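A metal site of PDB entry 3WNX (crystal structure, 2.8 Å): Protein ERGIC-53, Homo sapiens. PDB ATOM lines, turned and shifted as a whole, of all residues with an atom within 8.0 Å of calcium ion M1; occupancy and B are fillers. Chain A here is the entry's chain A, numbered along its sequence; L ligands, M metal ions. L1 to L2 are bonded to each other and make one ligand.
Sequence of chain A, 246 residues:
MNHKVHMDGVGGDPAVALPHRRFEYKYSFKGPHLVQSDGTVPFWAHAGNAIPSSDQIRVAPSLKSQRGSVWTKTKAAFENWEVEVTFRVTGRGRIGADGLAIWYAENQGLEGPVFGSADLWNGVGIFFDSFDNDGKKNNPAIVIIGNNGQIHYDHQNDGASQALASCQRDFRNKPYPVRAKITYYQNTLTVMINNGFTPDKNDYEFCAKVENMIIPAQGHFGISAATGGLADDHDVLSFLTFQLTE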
ATOM      1  N   GLY A  96       8.256 -35.173   8.955  1.00  0.00           N
ATOM      2  CA  GLY A  96       8.298 -35.346  10.407  1.00  0.00           C
ATOM      3  C   GLY A  96       9.061 -34.229  11.101  1.00  0.00           C
ATOM      4  O   GLY A  96       9.588 -33.320  10.456  1.00  0.00           O
ATOM      5  N   ALA A  97       9.133 -34.294  12.425  1.00  0.00           N
ATOM      6  CA  ALA A  97       9.744 -33.198  13.192  1.00  0.00           C
ATOM      7  C   ALA A  97      10.032 -33.626  14.618  1.00  0.00           C
ATOM      8  O   ALA A  97       9.524 -34.662  15.051  1.00  0.00           O
ATOM      9  CB  ALA A  97       8.808 -31.992  13.191  1.00  0.00           C
ATOM     10  N   ASP A  98      10.844 -32.863  15.357  1.00  0.00           N
ATOM     11  CA  ASP A  98      11.658 -31.767  14.803  1.00  0.00           C
ATOM     12  C   ASP A  98      13.066 -32.219  14.502  1.00  0.00           C
ATOM     13  O   ASP A  98      13.712 -31.721  13.572  1.00  0.00           O
ATOM     14  CB  ASP A  98      11.717 -30.574  15.767  1.00  0.00           C
ATOM     15  CG  ASP A  98      10.725 -29.496  15.410  1.00  0.00           C
ATOM     16  OD1 ASP A  98      10.124 -28.909  16.340  1.00  0.00           O
ATOM     17  OD2 ASP A  98      10.555 -29.244  14.185  1.00  0.00           O
ATOM     18  N   GLY A  99      13.540 -33.172  15.301  1.00  0.00           N
ATOM     19  CA  GLY A  99      14.790 -33.837  15.049  1.00  0.00           C
ATOM     20  C   GLY A  99      15.609 -34.020  16.296  1.00  0.00           C
ATOM     21  O   GLY A  99      15.148 -33.746  17.407  1.00  0.00           O
ATOM     22  N   PHE A 115      16.416 -28.211  20.277  1.00  0.00           N
ATOM     23  CA  PHE A 115      16.156 -29.653  20.198  1.00  0.00           C
ATOM     24  C   PHE A 115      16.012 -30.278  21.588  1.00  0.00           C
ATOM     25  O   PHE A 115      16.629 -31.292  21.883  1.00  0.00           O
ATOM     26  CB  PHE A 115      17.266 -30.325  19.389  1.00  0.00           C
ATOM     27  CG  PHE A 115      17.283 -29.923  17.954  1.00  0.00           C
ATOM     28  CD1 PHE A 115      16.800 -30.781  16.981  1.00  0.00           C
ATOM     29  CD2 PHE A 115      17.760 -28.676  17.559  1.00  0.00           C
ATOM     30  CE1 PHE A 115      16.792 -30.412  15.643  1.00  0.00           C
ATOM     31  CE2 PHE A 115      17.754 -28.304  16.231  1.00  0.00           C
ATOM     32  CZ  PHE A 115      17.271 -29.178  15.275  1.00  0.00           C
ATOM     33  N   PHE A 127      23.046 -31.684  14.609  1.00  0.00           N
ATOM     34  CA  PHE A 127      21.624 -31.638  14.605  1.00  0.00           C
ATOM     35  C   PHE A 127      21.141 -32.430  13.440  1.00  0.00           C
ATOM     36  O   PHE A 127      21.563 -32.218  12.307  1.00  0.00           O
ATOM     37  CB  PHE A 127      21.156 -30.204  14.505  1.00  0.00           C
ATOM     38  CG  PHE A 127      21.626 -29.346  15.648  1.00  0.00           C
ATOM     39  CD1 PHE A 127      22.116 -29.906  16.824  1.00  0.00           C
ATOM     40  CD2 PHE A 127      21.554 -27.966  15.557  1.00  0.00           C
ATOM     41  CE1 PHE A 127      22.539 -29.096  17.877  1.00  0.00           C
ATOM     42  CE2 PHE A 127      21.962 -27.160  16.605  1.00  0.00           C
ATOM     43  CZ  PHE A 127      22.454 -27.716  17.767  1.00  0.00           C
ATOM     44  N   PHE A 128      20.249 -33.363  13.753  1.00  0.00           N
ATOM     45  CA  PHE A 128      19.574 -34.144  12.760  1.00  0.00           C
ATOM     46  C   PHE A 128      18.223 -33.499  12.528  1.00  0.00           C
ATOM     47  O   PHE A 128      17.228 -33.916  13.115  1.00  0.00           O
ATOM     48  CB  PHE A 128      19.484 -35.574  13.261  1.00  0.00           C
ATOM     49  CG  PHE A 128      20.814 -36.229  13.426  1.00  0.00           C
ATOM     50  CD1 PHE A 128      21.307 -37.080  12.451  1.00  0.00           C
ATOM     51  CD2 PHE A 128      21.605 -35.964  14.530  1.00  0.00           C
ATOM     52  CE1 PHE A 128      22.563 -37.669  12.589  1.00  0.00           C
ATOM     53  CE2 PHE A 128      22.853 -36.564  14.686  1.00  0.00           C
ATOM     54  CZ  PHE A 128      23.329 -37.420  13.706  1.00  0.00           C
ATOM     55  N   ASP A 129      18.199 -32.478  11.663  1.00  0.00           N
ATOM     56  CA  ASP A 129      17.020 -31.633  11.449  1.00  0.00           C
ATOM     57  C   ASP A 129      16.056 -32.301  10.494  1.00  0.00           C
ATOM     58  O   ASP A 129      16.255 -32.289   9.280  1.00  0.00           O
ATOM     59  CB  ASP A 129      17.448 -30.269  10.912  1.00  0.00           C
ATOM     60  CG  ASP A 129      16.377 -29.194  11.032  1.00  0.00           C
ATOM     61  OD1 ASP A 129      15.170 -29.480  10.808  1.00  0.00           O
ATOM     62  OD2 ASP A 129      16.736 -28.036  11.359  1.00  0.00           O
ATOM     63  N   SER A 130      15.003 -32.913  11.051  1.00  0.00           N
ATOM     64  CA  SER A 130      13.956 -33.540  10.248  1.00  0.00           C
ATOM     65  C   SER A 130      13.176 -32.479   9.482  1.00  0.00           C
ATOM     66  O   SER A 130      12.793 -32.699   8.334  1.00  0.00           O
ATOM     67  CB  SER A 130      12.953 -34.318  11.121  1.00  0.00           C
ATOM     68  OG  SER A 130      13.590 -35.117  12.103  1.00  0.00           O
ATOM     69  N   PHE A 131      12.930 -31.347  10.145  1.00  0.00           N
ATOM     70  CA  PHE A 131      11.974 -30.372   9.618  1.00  0.00           C
ATOM     71  C   PHE A 131      12.600 -29.161   8.907  1.00  0.00           C
ATOM     72  O   PHE A 131      13.379 -28.376   9.480  1.00  0.00           O
ATOM     73  CB  PHE A 131      11.019 -29.893  10.712  1.00  0.00           C
ATOM     74  CG  PHE A 131       9.845 -29.128  10.161  1.00  0.00           C
ATOM     75  CD1 PHE A 131       8.967 -29.728   9.267  1.00  0.00           C
ATOM     76  CD2 PHE A 131       9.628 -27.789  10.515  1.00  0.00           C
ATOM     77  CE1 PHE A 131       7.884 -29.026   8.748  1.00  0.00           C
ATOM     78  CE2 PHE A 131       8.553 -27.076  10.000  1.00  0.00           C
ATOM     79  CZ  PHE A 131       7.673 -27.697   9.114  1.00  0.00           C
ATOM     80  N   ASP A 132      12.190 -29.031   7.642  1.00  0.00           N
ATOM     81  CA  ASP A 132      12.618 -27.987   6.729  1.00  0.00           C
ATOM     82  C   ASP A 132      12.147 -26.573   7.170  1.00  0.00           C
ATOM     83  O   ASP A 132      11.249 -25.989   6.545  1.00  0.00           O
ATOM     84  CB  ASP A 132      12.064 -28.338   5.336  1.00  0.00           C
ATOM     85  CG  ASP A 132      12.599 -27.453   4.244  1.00  0.00           C
ATOM     86  OD1 ASP A 132      13.787 -27.059   4.322  1.00  0.00           O
ATOM     87  OD2 ASP A 132      11.843 -27.167   3.295  1.00  0.00           O
ATOM     88  N   ASN A 133      12.763 -26.022   8.213  1.00  0.00           N
ATOM     89  CA  ASN A 133      12.228 -24.810   8.861  1.00  0.00           C
ATOM     90  C   ASN A 133      12.370 -23.495   8.069  1.00  0.00           C
ATOM     91  O   ASN A 133      11.553 -22.582   8.258  1.00  0.00           O
ATOM     92  CB  ASN A 133      12.795 -24.625  10.270  1.00  0.00           C
ATOM     93  CG  ASN A 133      12.303 -25.689  11.231  1.00  0.00           C
ATOM     94  OD1 ASN A 133      12.660 -26.870  11.109  1.00  0.00           O
ATOM     95  ND2 ASN A 133      11.498 -25.292  12.214  1.00  0.00           N
ATOM     96  N   ASP A 134      13.391 -23.382   7.215  1.00  0.00           N
ATOM     97  CA  ASP A 134      13.532 -22.204   6.332  1.00  0.00           C
ATOM     98  C   ASP A 134      12.925 -22.459   4.940  1.00  0.00           C
ATOM     99  O   ASP A 134      13.274 -21.790   3.972  1.00  0.00           O
ATOM    100  CB  ASP A 134      14.986 -21.704   6.249  1.00  0.00           C
ATOM    101  CG  ASP A 134      16.019 -22.830   6.158  1.00  0.00           C
ATOM    102  OD1 ASP A 134      15.802 -23.765   5.362  1.00  0.00           O
ATOM    103  OD2 ASP A 134      17.045 -22.769   6.865  1.00  0.00           O
ATOM    104  N   ASN A 138      15.830 -28.411   1.915  1.00  0.00           N
ATOM    105  CA  ASN A 138      17.169 -28.903   2.203  1.00  0.00           C
ATOM    106  C   ASN A 138      17.174 -29.950   3.326  1.00  0.00           C
ATOM    107  O   ASN A 138      18.241 -30.356   3.835  1.00  0.00           O
ATOM    108  CB  ASN A 138      18.083 -27.735   2.613  1.00  0.00           C
ATOM    109  CG  ASN A 138      17.606 -27.064   3.886  1.00  0.00           C
ATOM    110  OD1 ASN A 138      16.408 -26.815   4.062  1.00  0.00           O
ATOM    111  ND2 ASN A 138      18.527 -26.774   4.799  1.00  0.00           N
ATOM    112  N   ASN A 139      15.981 -30.366   3.736  1.00  0.00           N
ATOM    113  CA  ASN A 139      15.826 -31.293   4.837  1.00  0.00           C
ATOM    114  C   ASN A 139      15.319 -32.650   4.362  1.00  0.00           C
ATOM    115  O   ASN A 139      14.812 -32.734   3.241  1.00  0.00           O
ATOM    116  CB  ASN A 139      14.931 -30.664   5.911  1.00  0.00           C
ATOM    117  CG  ASN A 139      15.693 -29.682   6.769  1.00  0.00           C
ATOM    118  OD1 ASN A 139      16.697 -29.120   6.345  1.00  0.00           O
ATOM    119  ND2 ASN A 139      15.255 -29.495   7.996  1.00  0.00           N
ATOM    120  N   ALA A 141      18.458 -33.188   7.208  1.00  0.00           N
ATOM    121  CA  ALA A 141      19.882 -32.931   7.049  1.00  0.00           C
ATOM    122  C   ALA A 141      20.611 -32.965   8.386  1.00  0.00           C
ATOM    123  O   ALA A 141      20.023 -32.680   9.429  1.00  0.00           O
ATOM    124  CB  ALA A 141      20.079 -31.577   6.393  1.00  0.00           C
ATOM    125  N   TYR A 153      20.807 -20.295  18.570  1.00  0.00           N
ATOM    126  CA  TYR A 153      20.623 -21.186  17.426  1.00  0.00           C
ATOM    127  C   TYR A 153      19.472 -20.694  16.563  1.00  0.00           C
ATOM    128  O   TYR A 153      18.338 -20.559  17.043  1.00  0.00           O
ATOM    129  CB  TYR A 153      20.381 -22.636  17.866  1.00  0.00           C
ATOM    130  CG  TYR A 153      19.725 -23.475  16.801  1.00  0.00           C
ATOM    131  CD1 TYR A 153      20.398 -23.798  15.638  1.00  0.00           C
ATOM    132  CD2 TYR A 153      18.420 -23.925  16.945  1.00  0.00           C
ATOM    133  CE1 TYR A 153      19.798 -24.563  14.651  1.00  0.00           C
ATOM    134  CE2 TYR A 153      17.804 -24.694  15.975  1.00  0.00           C
ATOM    135  CZ  TYR A 153      18.495 -25.010  14.826  1.00  0.00           C
ATOM    136  OH  TYR A 153      17.878 -25.762  13.839  1.00  0.00           O
ATOM    137  N   ASP A 154      19.752 -20.440  15.300  1.00  0.00           N
ATOM    138  CA  ASP A 154      18.737 -19.931  14.426  1.00  0.00           C
ATOM    139  C   ASP A 154      17.852 -21.094  14.061  1.00  0.00           C
ATOM    140  O   ASP A 154      18.056 -21.763  13.053  1.00  0.00           O
ATOM    141  CB  ASP A 154      19.342 -19.289  13.175  1.00  0.00           C
ATOM    142  CG  ASP A 154      18.315 -18.545  12.357  1.00  0.00           C
ATOM    143  OD1 ASP A 154      17.121 -18.930  12.378  1.00  0.00           O
ATOM    144  OD2 ASP A 154      18.687 -17.559  11.672  1.00  0.00           O
ATOM    145  N   HIS A 155      16.861 -21.335  14.922  1.00  0.00           N
ATOM    146  CA  HIS A 155      15.942 -22.459  14.763  1.00  0.00           C
ATOM    147  C   HIS A 155      15.209 -22.395  13.426  1.00  0.00           C
ATOM    148  O   HIS A 155      15.267 -23.345  12.646  1.00  0.00           O
ATOM    149  CB  HIS A 155      14.931 -22.525  15.917  1.00  0.00           C
ATOM    150  CG  HIS A 155      14.113 -23.779  15.923  1.00  0.00           C
ATOM    151  ND1 HIS A 155      14.379 -24.845  16.759  1.00  0.00           N
ATOM    152  CD2 HIS A 155      13.027 -24.139  15.194  1.00  0.00           C
ATOM    153  CE1 HIS A 155      13.494 -25.805  16.549  1.00  0.00           C
ATOM    154  NE2 HIS A 155      12.660 -25.406  15.600  1.00  0.00           N
ATOM    155  N   GLN A 156      14.557 -21.261  13.173  1.00  0.00           N
ATOM    156  CA  GLN A 156      13.714 -21.095  11.984  1.00  0.00           C
ATOM    157  C   GLN A 156      14.508 -21.238  10.695  1.00  0.00           C
ATOM    158  O   GLN A 156      13.933 -21.615   9.672  1.00  0.00           O
ATOM    159  CB  GLN A 156      12.980 -19.750  11.982  1.00  0.00           C
ATOM    160  CG  GLN A 156      11.879 -19.602  13.035  1.00  0.00           C
ATOM    161  CD  GLN A 156      12.319 -18.818  14.271  1.00  0.00           C
ATOM    162  OE1 GLN A 156      13.490 -18.815  14.648  1.00  0.00           O
ATOM    163  NE2 GLN A 156      11.358 -18.147  14.916  1.00  0.00           N
ATOM    164  N   ASN A 157      15.805 -20.948  10.736  1.00  0.00           N
ATOM    165  CA  ASN A 157      16.683 -21.112   9.564  1.00  0.00           C
ATOM    166  C   ASN A 157      17.584 -22.348   9.632  1.00  0.00           C
ATOM    167  O   ASN A 157      18.658 -22.363   9.023  1.00  0.00           O
ATOM    168  CB  ASN A 157      17.536 -19.862   9.339  1.00  0.00           C
ATOM    169  CG  ASN A 157      16.706 -18.665   8.901  1.00  0.00           C
ATOM    170  OD1 ASN A 157      15.914 -18.765   7.955  1.00  0.00           O
ATOM    171  ND2 ASN A 157      16.887 -17.528   9.575  1.00  0.00           N
ATOM    172  N   ASP A 158      17.148 -23.371  10.361  1.00  0.00           N
ATOM    173  CA  ASP A 158      17.942 -24.565  10.576  1.00  0.00           C
ATOM    174  C   ASP A 158      19.357 -24.266  11.080  1.00  0.00           C
ATOM    175  O   ASP A 158      20.160 -25.181  11.195  1.00  0.00           O
ATOM    176  CB  ASP A 158      18.067 -25.376   9.279  1.00  0.00           C
ATOM    177  CG  ASP A 158      16.737 -25.663   8.624  1.00  0.00           C
ATOM    178  OD1 ASP A 158      15.689 -25.529   9.279  1.00  0.00           O
ATOM    179  OD2 ASP A 158      16.755 -26.030   7.430  1.00  0.00           O
ATOM    180  N   GLY A 159      19.671 -23.002  11.367  1.00  0.00           N
ATOM    181  CA  GLY A 159      21.055 -22.578  11.532  1.00  0.00           C
ATOM    182  C   GLY A 159      21.952 -22.716  10.289  1.00  0.00           C
ATOM    183  O   GLY A 159      23.181 -22.805  10.420  1.00  0.00           O
HETATM  184  C1  LIG L   1       5.386 -25.722  13.977  1.00  0.00           C
HETATM  185  C2  LIG L   1       6.398 -24.891  14.800  1.00  0.00           C
HETATM  186  C3  LIG L   1       7.855 -25.026  14.373  1.00  0.00           C
HETATM  187  C4  LIG L   1       8.179 -26.487  14.158  1.00  0.00           C
HETATM  188  C5  LIG L   1       7.150 -27.158  13.256  1.00  0.00           C
HETATM  189  C6  LIG L   1       7.390 -28.665  13.160  1.00  0.00           C
HETATM  190  O1  LIG L   1       5.080 -25.150  12.701  1.00  0.00           O
HETATM  191  O2  LIG L   1       6.425 -25.268  16.169  1.00  0.00           O
HETATM  192  O3  LIG L   1       8.707 -24.561  15.405  1.00  0.00           O
HETATM  193  O4  LIG L   1       9.472 -26.542  13.592  1.00  0.00           O
HETATM  194  O5  LIG L   1       5.850 -27.029  13.774  1.00  0.00           O
HETATM  195  O6  LIG L   1       7.144 -29.277  14.420  1.00  0.00           O
HETATM  196  C1  LG2 L   2       6.277 -24.120  17.031  1.00  0.00           C
HETATM  197  C2  LG2 L   2       6.715 -24.480  18.454  1.00  0.00           C
HETATM  198  C3  LG2 L   2       5.708 -25.484  19.060  1.00  0.00           C
HETATM  199  C4  LG2 L   2       4.238 -25.100  18.752  1.00  0.00           C
HETATM  200  C5  LG2 L   2       4.052 -24.770  17.268  1.00  0.00           C
HETATM  201  C6  LG2 L   2       2.621 -24.385  16.826  1.00  0.00           C
HETATM  202  O1  LG2 L   2       6.905 -23.313  19.258  1.00  0.00           O
HETATM  203  O2  LG2 L   2       5.911 -25.708  20.442  1.00  0.00           O
HETATM  204  O3  LG2 L   2       3.440 -26.192  19.100  1.00  0.00           O
HETATM  205  O4  LG2 L   2       4.940 -23.691  17.011  1.00  0.00           O
HETATM  206  O5  LG2 L   2       2.313 -24.908  15.541  1.00  0.00           O
HETATM  207 CA    CA M   1      14.596 -27.397  11.641  1.00  0.00          CA
HETATM  208 CA    CA M   2      15.491 -26.264   5.972  1.00  0.00          CA
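N of Asn 133 sits at hydrogen-bond distance from OD1 of Asp 158 (3.2 Å).
The backbone carbonyl oxygen of Asp 129 lies within hydrogen-bond range of the side-chain amide nitrogen of Asn 139, at 3.2 Å.
The backbone carbonyl oxygen of Ala 141 is in hydrogen-bond range of the backbone NH of Asp 129 (2.9 Å).
The side-chain amide nitrogen of Asn 139 lies close to the backbone carbonyl oxygen of Phe 131.
The side-chain carboxylate of Asp 158 lies close to the side-chain amide oxygen of Asn 139 (3.3 Å).
Merely in contact with calcium ion M1: Asp 158 (3.2 Å).
Along chain A the residues within 4 Å of calcium ion M1 span positions 129 to 158.
The nearest printed residue that does not touch calcium ion M1 is His 155 (4.2 Å).
Calcium ion M1 is bound by the side-chain amide oxygen (OD1) of Asn 133 (2.1 Å), the side-chain carboxylate (OD2) of Asp 129 (2.3 Å), the side-chain carboxylate (OD1) of Asp 129 (2.3 Å) and the backbone carbonyl oxygen (O) of Phe 131 (2.7 Å).
ND2 of Asn 133 lies within hydrogen-bond range of O4 of LIG L1 (2.8 Å).
The side-chain carboxylate of Asp 98 is in hydrogen-bond range of an oxygen (O4) of LIG L1, 3.0 Å away.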
